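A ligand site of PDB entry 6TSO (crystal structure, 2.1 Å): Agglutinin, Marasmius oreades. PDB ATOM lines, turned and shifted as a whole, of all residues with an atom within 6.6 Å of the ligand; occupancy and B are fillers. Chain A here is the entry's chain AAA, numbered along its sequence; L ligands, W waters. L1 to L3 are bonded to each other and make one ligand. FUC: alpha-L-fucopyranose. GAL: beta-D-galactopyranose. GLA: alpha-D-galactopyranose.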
ATOM      1  N   HIS A   9      -7.270   2.464 -23.588  1.00  0.00           N
ATOM      2  CA  HIS A   9      -7.729   3.868 -23.729  1.00  0.00           C
ATOM      3  C   HIS A   9      -9.134   3.760 -24.306  1.00  0.00           C
ATOM      4  O   HIS A   9      -9.260   3.244 -25.444  1.00  0.00           O
ATOM      5  CB  HIS A   9      -6.710   4.667 -24.540  1.00  0.00           C
ATOM      6  CG  HIS A   9      -6.937   6.129 -24.521  1.00  0.00           C
ATOM      7  ND1 HIS A   9      -7.319   6.821 -25.650  1.00  0.00           N
ATOM      8  CD2 HIS A   9      -6.882   7.034 -23.507  1.00  0.00           C
ATOM      9  CE1 HIS A   9      -7.469   8.098 -25.338  1.00  0.00           C
ATOM     10  NE2 HIS A   9      -7.220   8.248 -24.012  1.00  0.00           N
ATOM     11  N   ASP A  20     -12.220   9.335 -18.581  1.00  0.00           N
ATOM     12  CA  ASP A  20     -11.183  10.100 -17.876  1.00  0.00           C
ATOM     13  C   ASP A  20     -11.636  10.209 -16.420  1.00  0.00           C
ATOM     14  O   ASP A  20     -12.757  10.634 -16.166  1.00  0.00           O
ATOM     15  CB  ASP A  20     -10.960  11.439 -18.594  1.00  0.00           C
ATOM     16  CG  ASP A  20      -9.943  12.366 -17.963  1.00  0.00           C
ATOM     17  OD1 ASP A  20     -10.143  12.781 -16.779  1.00  0.00           O
ATOM     18  OD2 ASP A  20      -8.967  12.696 -18.655  1.00  0.00           O
ATOM     19  N   LEU A  21     -10.809   9.787 -15.483  1.00  0.00           N
ATOM     20  CA  LEU A  21     -11.082   9.981 -14.052  1.00  0.00           C
ATOM     21  C   LEU A  21     -10.560  11.368 -13.721  1.00  0.00           C
ATOM     22  O   LEU A  21      -9.353  11.612 -13.847  1.00  0.00           O
ATOM     23  CB  LEU A  21     -10.382   8.866 -13.285  1.00  0.00           C
ATOM     24  CG  LEU A  21     -10.444   8.993 -11.779  1.00  0.00           C
ATOM     25  CD1 LEU A  21     -11.865   8.788 -11.262  1.00  0.00           C
ATOM     26  CD2 LEU A  21      -9.498   7.986 -11.140  1.00  0.00           C
ATOM     27  N   LYS A  22     -11.462  12.278 -13.369  1.00  0.00           N
ATOM     28  CA  LYS A  22     -11.151  13.736 -13.381  1.00  0.00           C
ATOM     29  C   LYS A  22      -9.944  13.992 -12.449  1.00  0.00           C
ATOM     30  O   LYS A  22      -9.990  13.579 -11.290  1.00  0.00           O
ATOM     31  CB  LYS A  22     -12.403  14.509 -12.980  1.00  0.00           C
ATOM     32  CG  LYS A  22     -12.394  15.909 -13.565  1.00  0.00           C
ATOM     33  CD  LYS A  22     -13.621  16.717 -13.316  1.00  0.00           C
ATOM     34  CE  LYS A  22     -13.342  18.160 -13.668  1.00  0.00           C
ATOM     35  NZ  LYS A  22     -14.501  19.022 -13.368  1.00  0.00           N
ATOM     36  N   ASP A  23      -8.911  14.640 -12.968  1.00  0.00           N
ATOM     37  CA  ASP A  23      -7.652  15.031 -12.249  1.00  0.00           C
ATOM     38  C   ASP A  23      -6.939  13.778 -11.736  1.00  0.00           C
ATOM     39  O   ASP A  23      -5.996  13.908 -10.943  1.00  0.00           O
ATOM     40  CB  ASP A  23      -7.917  16.021 -11.111  1.00  0.00           C
ATOM     41  CG  ASP A  23      -6.714  16.882 -10.732  1.00  0.00           C
ATOM     42  OD1 ASP A  23      -6.026  17.387 -11.645  1.00  0.00           O
ATOM     43  OD2 ASP A  23      -6.448  17.032  -9.515  1.00  0.00           O
ATOM     44  N   GLY A  24      -7.286  12.586 -12.214  1.00  0.00           N
ATOM     45  CA  GLY A  24      -6.660  11.336 -11.776  1.00  0.00           C
ATOM     46  C   GLY A  24      -6.825  11.114 -10.277  1.00  0.00           C
ATOM     47  O   GLY A  24      -6.042  10.301  -9.717  1.00  0.00           O
ATOM     48  N   VAL A  33     -15.463  11.222 -16.501  1.00  0.00           N
ATOM     49  CA  VAL A  33     -16.065  12.176 -17.472  1.00  0.00           C
ATOM     50  C   VAL A  33     -15.441  11.924 -18.841  1.00  0.00           C
ATOM     51  O   VAL A  33     -14.376  11.281 -18.916  1.00  0.00           O
ATOM     52  CB  VAL A  33     -15.853  13.629 -17.005  1.00  0.00           C
ATOM     53  CG1 VAL A  33     -16.478  13.881 -15.636  1.00  0.00           C
ATOM     54  CG2 VAL A  33     -14.383  14.027 -16.979  1.00  0.00           C
ATOM     55  N   TRP A  35     -13.265  13.440 -21.877  1.00  0.00           N
ATOM     56  CA  TRP A  35     -12.174  14.416 -22.029  1.00  0.00           C
ATOM     57  C   TRP A  35     -11.445  14.122 -23.331  1.00  0.00           C
ATOM     58  O   TRP A  35     -11.352  12.944 -23.685  1.00  0.00           O
ATOM     59  CB  TRP A  35     -11.226  14.381 -20.809  1.00  0.00           C
ATOM     60  CG  TRP A  35     -10.597  15.689 -20.496  1.00  0.00           C
ATOM     61  CD1 TRP A  35      -9.543  16.287 -21.135  1.00  0.00           C
ATOM     62  CD2 TRP A  35     -11.011  16.615 -19.459  1.00  0.00           C
ATOM     63  NE1 TRP A  35      -9.231  17.481 -20.532  1.00  0.00           N
ATOM     64  CE2 TRP A  35     -10.141  17.727 -19.536  1.00  0.00           C
ATOM     65  CE3 TRP A  35     -11.980  16.584 -18.452  1.00  0.00           C
ATOM     66  CZ2 TRP A  35     -10.259  18.817 -18.668  1.00  0.00           C
ATOM     67  CZ3 TRP A  35     -12.075  17.656 -17.592  1.00  0.00           C
ATOM     68  CH2 TRP A  35     -11.204  18.741 -17.682  1.00  0.00           C
ATOM     69  N   GLN A  36     -10.968  15.149 -24.021  1.00  0.00           N
ATOM     70  CA  GLN A  36     -10.187  14.985 -25.270  1.00  0.00           C
ATOM     71  C   GLN A  36      -8.840  14.364 -24.898  1.00  0.00           C
ATOM     72  O   GLN A  36      -8.480  14.336 -23.723  1.00  0.00           O
ATOM     73  CB  GLN A  36     -10.003  16.330 -26.000  1.00  0.00           C
ATOM     74  CG  GLN A  36      -9.234  17.354 -25.200  1.00  0.00           C
ATOM     75  CD  GLN A  36      -9.143  18.652 -25.955  1.00  0.00           C
ATOM     76  OE1 GLN A  36      -8.631  18.677 -27.080  1.00  0.00           O
ATOM     77  NE2 GLN A  36      -9.723  19.710 -25.372  1.00  0.00           N
ATOM     78  N   PHE A  37      -8.103  13.886 -25.890  1.00  0.00           N
ATOM     79  CA  PHE A  37      -6.855  13.148 -25.669  1.00  0.00           C
ATOM     80  C   PHE A  37      -5.893  13.441 -26.808  1.00  0.00           C
ATOM     81  O   PHE A  37      -6.304  14.032 -27.811  1.00  0.00           O
ATOM     82  CB  PHE A  37      -7.231  11.660 -25.559  1.00  0.00           C
ATOM     83  CG  PHE A  37      -7.979  11.127 -26.739  1.00  0.00           C
ATOM     84  CD1 PHE A  37      -7.306  10.544 -27.793  1.00  0.00           C
ATOM     85  CD2 PHE A  37      -9.364  11.065 -26.711  1.00  0.00           C
ATOM     86  CE1 PHE A  37      -8.008   9.996 -28.854  1.00  0.00           C
ATOM     87  CE2 PHE A  37     -10.068  10.489 -27.761  1.00  0.00           C
ATOM     88  CZ  PHE A  37      -9.386   9.975 -28.839  1.00  0.00           C
ATOM     89  N   THR A  38      -4.632  13.062 -26.625  1.00  0.00           N
ATOM     90  CA  THR A  38      -3.585  13.244 -27.656  1.00  0.00           C
ATOM     91  C   THR A  38      -3.117  11.828 -27.988  1.00  0.00           C
ATOM     92  O   THR A  38      -2.684  11.108 -27.106  1.00  0.00           O
ATOM     93  CB  THR A  38      -2.469  14.181 -27.191  1.00  0.00           C
ATOM     94  OG1 THR A  38      -3.012  15.314 -26.513  1.00  0.00           O
ATOM     95  CG2 THR A  38      -1.631  14.718 -28.329  1.00  0.00           C
ATOM     96  N   PRO A  39      -3.214  11.395 -29.262  1.00  0.00           N
ATOM     97  CA  PRO A  39      -2.643  10.120 -29.686  1.00  0.00           C
ATOM     98  C   PRO A  39      -1.129  10.046 -29.425  1.00  0.00           C
ATOM     99  O   PRO A  39      -0.517  11.084 -29.418  1.00  0.00           O
ATOM    100  CB  PRO A  39      -2.883  10.071 -31.207  1.00  0.00           C
ATOM    101  CG  PRO A  39      -3.987  11.090 -31.442  1.00  0.00           C
ATOM    102  CD  PRO A  39      -3.789  12.152 -30.375  1.00  0.00           C
ATOM    103  N   THR A  41       0.663   9.564 -26.919  1.00  0.00           N
ATOM    104  CA  THR A  41       1.099  10.064 -25.605  1.00  0.00           C
ATOM    105  C   THR A  41       0.621   9.080 -24.542  1.00  0.00           C
ATOM    106  O   THR A  41      -0.201   8.177 -24.843  1.00  0.00           O
ATOM    107  CB  THR A  41       0.580  11.467 -25.250  1.00  0.00           C
ATOM    108  OG1 THR A  41      -0.857  11.465 -25.146  1.00  0.00           O
ATOM    109  CG2 THR A  41       0.992  12.526 -26.266  1.00  0.00           C
ATOM    110  N   ILE A  42       1.135   9.262 -23.330  1.00  0.00           N
ATOM    111  CA  ILE A  42       0.533   8.732 -22.085  1.00  0.00           C
ATOM    112  C   ILE A  42      -0.602   9.676 -21.723  1.00  0.00           C
ATOM    113  O   ILE A  42      -0.294  10.843 -21.436  1.00  0.00           O
ATOM    114  CB  ILE A  42       1.608   8.613 -20.980  1.00  0.00           C
ATOM    115  CG1 ILE A  42       2.682   7.585 -21.378  1.00  0.00           C
ATOM    116  CG2 ILE A  42       0.975   8.312 -19.633  1.00  0.00           C
ATOM    117  CD1 ILE A  42       2.130   6.252 -21.878  1.00  0.00           C
ATOM    118  N   ASN A  43      -1.867   9.238 -21.878  1.00  0.00           N
ATOM    119  CA  ASN A  43      -3.054  10.001 -21.410  1.00  0.00           C
ATOM    120  C   ASN A  43      -3.267   9.590 -19.939  1.00  0.00           C
ATOM    121  O   ASN A  43      -3.934   8.586 -19.671  1.00  0.00           O
ATOM    122  CB  ASN A  43      -4.242   9.768 -22.342  1.00  0.00           C
ATOM    123  CG  ASN A  43      -3.992  10.426 -23.678  1.00  0.00           C
ATOM    124  OD1 ASN A  43      -4.001  11.652 -23.737  1.00  0.00           O
ATOM    125  ND2 ASN A  43      -3.762   9.633 -24.722  1.00  0.00           N
ATOM    126  N   TRP A  44      -2.586  10.315 -19.067  1.00  0.00           N
ATOM    127  CA  TRP A  44      -2.314   9.955 -17.650  1.00  0.00           C
ATOM    128  C   TRP A  44      -3.585   9.578 -16.860  1.00  0.00           C
ATOM    129  O   TRP A  44      -3.460   8.709 -15.946  1.00  0.00           O
ATOM    130  CB  TRP A  44      -1.598  11.116 -16.962  1.00  0.00           C
ATOM    131  CG  TRP A  44      -0.129  11.103 -17.253  1.00  0.00           C
ATOM    132  CD1 TRP A  44       0.527  11.843 -18.185  1.00  0.00           C
ATOM    133  CD2 TRP A  44       0.849  10.208 -16.679  1.00  0.00           C
ATOM    134  NE1 TRP A  44       1.850  11.508 -18.190  1.00  0.00           N
ATOM    135  CE2 TRP A  44       2.075  10.511 -17.284  1.00  0.00           C
ATOM    136  CE3 TRP A  44       0.791   9.236 -15.682  1.00  0.00           C
ATOM    137  CZ2 TRP A  44       3.257   9.869 -16.924  1.00  0.00           C
ATOM    138  CZ3 TRP A  44       1.956   8.590 -15.336  1.00  0.00           C
ATOM    139  CH2 TRP A  44       3.175   8.895 -15.947  1.00  0.00           C
ATOM    140  N   HIS A  45      -4.735  10.192 -17.145  1.00  0.00           N
ATOM    141  CA  HIS A  45      -5.963   9.919 -16.336  1.00  0.00           C
ATOM    142  C   HIS A  45      -6.941   9.020 -17.085  1.00  0.00           C
ATOM    143  O   HIS A  45      -8.061   8.843 -16.563  1.00  0.00           O
ATOM    144  CB  HIS A  45      -6.627  11.238 -15.956  1.00  0.00           C
ATOM    145  CG  HIS A  45      -5.700  12.141 -15.241  1.00  0.00           C
ATOM    146  ND1 HIS A  45      -5.935  13.491 -15.180  1.00  0.00           N
ATOM    147  CD2 HIS A  45      -4.570  11.905 -14.537  1.00  0.00           C
ATOM    148  CE1 HIS A  45      -4.978  14.060 -14.450  1.00  0.00           C
ATOM    149  NE2 HIS A  45      -4.133  13.113 -14.040  1.00  0.00           N
ATOM    150  N   GLN A  46      -6.524   8.451 -18.223  1.00  0.00           N
ATOM    151  CA  GLN A  46      -7.472   7.884 -19.216  1.00  0.00           C
ATOM    152  C   GLN A  46      -7.083   6.416 -19.539  1.00  0.00           C
ATOM    153  O   GLN A  46      -7.592   5.920 -20.539  1.00  0.00           O
ATOM    154  CB  GLN A  46      -7.481   8.791 -20.458  1.00  0.00           C
ATOM    155  CG  GLN A  46      -7.978  10.236 -20.225  1.00  0.00           C
ATOM    156  CD  GLN A  46      -7.875  11.104 -21.474  1.00  0.00           C
ATOM    157  OE1 GLN A  46      -7.438  10.633 -22.517  1.00  0.00           O
ATOM    158  NE2 GLN A  46      -8.292  12.365 -21.405  1.00  0.00           N
ATOM    159  N   PHE A  66      -3.568   5.079 -13.120  1.00  0.00           N
ATOM    160  CA  PHE A  66      -3.019   6.209 -12.341  1.00  0.00           C
ATOM    161  C   PHE A  66      -3.512   6.180 -10.881  1.00  0.00           C
ATOM    162  O   PHE A  66      -2.682   6.288  -9.965  1.00  0.00           O
ATOM    163  CB  PHE A  66      -3.433   7.558 -12.936  1.00  0.00           C
ATOM    164  CG  PHE A  66      -2.699   8.695 -12.289  1.00  0.00           C
ATOM    165  CD1 PHE A  66      -1.326   8.765 -12.375  1.00  0.00           C
ATOM    166  CD2 PHE A  66      -3.378   9.652 -11.562  1.00  0.00           C
ATOM    167  CE1 PHE A  66      -0.623   9.806 -11.762  1.00  0.00           C
ATOM    168  CE2 PHE A  66      -2.697  10.694 -10.951  1.00  0.00           C
ATOM    169  CZ  PHE A  66      -1.315  10.761 -11.033  1.00  0.00           C
ATOM    170  N   ASP A 131     -14.932  18.851 -22.667  1.00  0.00           N
ATOM    171  CA  ASP A 131     -14.016  18.366 -21.605  1.00  0.00           C
ATOM    172  C   ASP A 131     -14.724  18.445 -20.256  1.00  0.00           C
ATOM    173  O   ASP A 131     -15.027  19.570 -19.854  1.00  0.00           O
ATOM    174  CB  ASP A 131     -12.731  19.184 -21.594  1.00  0.00           C
ATOM    175  CG  ASP A 131     -11.840  18.875 -22.774  1.00  0.00           C
ATOM    176  OD1 ASP A 131     -12.008  17.784 -23.351  1.00  0.00           O
ATOM    177  OD2 ASP A 131     -10.952  19.709 -23.095  1.00  0.00           O
HETATM  178  C1  FUC L   1      -2.714  16.485 -18.791  1.00  0.00           C
HETATM  179  C2  FUC L   1      -1.752  17.607 -19.186  1.00  0.00           C
HETATM  180  C3  FUC L   1      -1.153  18.222 -17.935  1.00  0.00           C
HETATM  181  C4  FUC L   1      -0.518  17.149 -17.098  1.00  0.00           C
HETATM  182  C5  FUC L   1      -1.552  16.104 -16.727  1.00  0.00           C
HETATM  183  C6  FUC L   1      -1.003  14.918 -15.960  1.00  0.00           C
HETATM  184  O2  FUC L   1      -2.477  18.558 -19.966  1.00  0.00           O
HETATM  185  O3  FUC L   1      -0.174  19.152 -18.327  1.00  0.00           O
HETATM  186  O4  FUC L   1       0.521  16.454 -17.813  1.00  0.00           O
HETATM  187  O5  FUC L   1      -2.093  15.535 -17.912  1.00  0.00           O
HETATM  188  C1  GAL L   2      -5.589  17.048 -16.620  1.00  0.00           C
HETATM  189  C2  GAL L   2      -4.934  16.271 -17.778  1.00  0.00           C
HETATM  190  C3  GAL L   2      -5.915  16.041 -18.923  1.00  0.00           C
HETATM  191  C4  GAL L   2      -7.194  15.438 -18.329  1.00  0.00           C
HETATM  192  C5  GAL L   2      -7.744  16.297 -17.171  1.00  0.00           C
HETATM  193  C6  GAL L   2      -8.948  15.619 -16.536  1.00  0.00           C
HETATM  194  O1  GAL L   2      -4.698  16.929 -15.567  1.00  0.00           O
HETATM  195  O2  GAL L   2      -3.789  17.034 -18.168  1.00  0.00           O
HETATM  196  O3  GAL L   2      -5.414  15.172 -20.000  1.00  0.00           O
HETATM  197  O4  GAL L   2      -6.911  14.082 -17.899  1.00  0.00           O
HETATM  198  O5  GAL L   2      -6.801  16.486 -16.143  1.00  0.00           O
HETATM  199  O6  GAL L   2      -8.498  14.536 -15.690  1.00  0.00           O
HETATM  200  C1  GLA L   3      -6.042  15.108 -21.164  1.00  0.00           C
HETATM  201  C2  GLA L   3      -5.199  14.308 -22.185  1.00  0.00           C
HETATM  202  C3  GLA L   3      -4.188  15.192 -22.943  1.00  0.00           C
HETATM  203  C4  GLA L   3      -4.852  16.485 -23.399  1.00  0.00           C
HETATM  204  C5  GLA L   3      -5.494  17.185 -22.178  1.00  0.00           C
HETATM  205  C6  GLA L   3      -6.080  18.522 -22.500  1.00  0.00           C
HETATM  206  O2  GLA L   3      -4.502  13.252 -21.509  1.00  0.00           O
HETATM  207  O3  GLA L   3      -3.648  14.398 -24.032  1.00  0.00           O
HETATM  208  O4  GLA L   3      -5.808  16.188 -24.413  1.00  0.00           O
HETATM  209  O5  GLA L   3      -6.522  16.335 -21.724  1.00  0.00           O
HETATM  210  O6  GLA L   3      -6.854  19.046 -21.402  1.00  0.00           O
HETATM  211  O   HOH W   1      -4.782  19.861 -19.421  1.00  0.00           O
HETATM  212  O   HOH W   2      -1.503  13.225 -23.166  1.00  0.00           O
HETATM  213  O   HOH W   3      -5.228  12.406 -19.231  1.00  0.00           O
HETATM  214  O   HOH W   4      -1.906  13.122 -19.983  1.00  0.00           O
HETATM  215  O   HOH W   5      -7.417  18.078 -13.883  1.00  0.00           O
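The side-chain carboxylate of Asp 20 is in hydrogen-bond range of an oxygen (O4) of GAL L2 (2.6 Å). An oxygen (O3) of GLA L3 lies within hydrogen-bond range of the backbone NH (N) of Thr 38. The side-chain hydroxyl of Thr 38 sits at hydrogen-bond distance from an oxygen (O3) of GLA L3, at 2.7 Å. The backbone NH (N) of Asp 23 sits at hydrogen-bond distance from an oxygen (O6) of GAL L2. The side-chain amide oxygen (OD1) of Asn 43 sits at hydrogen-bond distance from an oxygen (O3) of GLA L3 (2.8 Å). ND1 of His 45 sits at hydrogen-bond distance from O6 of GAL L2. The indole nitrogen (NE1) of Trp 35 sits at hydrogen-bond distance from an oxygen (O6) of GLA L3, 3.0 Å away. The backbone carbonyl oxygen (O) of Gln 36 sits at hydrogen-bond distance from an oxygen (O4) of GLA L3 (3.3 Å).
The side-chain carboxylate (OD2) of Asp 20 is in hydrogen-bond range of the side-chain amide nitrogen (NE2) of Gln 46 (2.9 Å). N of Val 33 is in hydrogen-bond range of O of Asp 20. O of Thr 38 lies within hydrogen-bond range of OG1 of Thr 41, at 2.7 Å. The backbone NH of Leu 21 lies within hydrogen-bond range of the backbone carbonyl oxygen of His 45, 3.1 Å away. A ring nitrogen (ND1) of His 45 sits at hydrogen-bond distance from the backbone NH (N) of Gly 24. O of Gln 36 lies within hydrogen-bond range of NE2 of Gln 46, 3.0 Å away. The side-chain carboxylate (OD2) of Asp 131 lies within hydrogen-bond range of the side-chain amide nitrogen (NE2) of Gln 36 (2.6 Å). The side-chain amide oxygen (OE1) of Gln 46 sits at hydrogen-bond distance from a ring nitrogen (NE2) of His 9 (2.8 Å).
Merely in contact with the ligand: Phe 37, Gln 46, Leu 21, Lys 22 and Trp 44. Hydrophobic or aromatic side chains within 4 Å of the ligand: Trp 35, Trp 44 and His 45. 12 residues have an atom within 4 Å of the ligand: Asp 20, Leu 21, Lys 22, Asp 23, Trp 35, Gln 36, Phe 37, Thr 38, Asn 43, Trp 44, His 45 and Gln 46.
Water W3 lies within hydrogen-bond range of an oxygen (O2) of GLA L3 (2.5 Å), the backbone NH (N) of His 45 (3.1 Å) and the backbone NH (N) of Trp 44 (3.4 Å). Water W2 lies within hydrogen-bond range of O3 of GLA L3 (2.6 Å), OG1 of Thr 41 (2.7 Å), OD1 of Asn 43 (3.0 Å) and O of Ile 42 (3.2 Å). Water W5 bridges OD1 of Asp 23 (2.7 Å) and O5 of GAL L2 (2.8 Å). Water W4 lies within hydrogen-bond range of O2 of GLA L3 (3.0 Å), N of Trp 44 (3.0 Å) and O of Ile 42 (3.1 Å).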
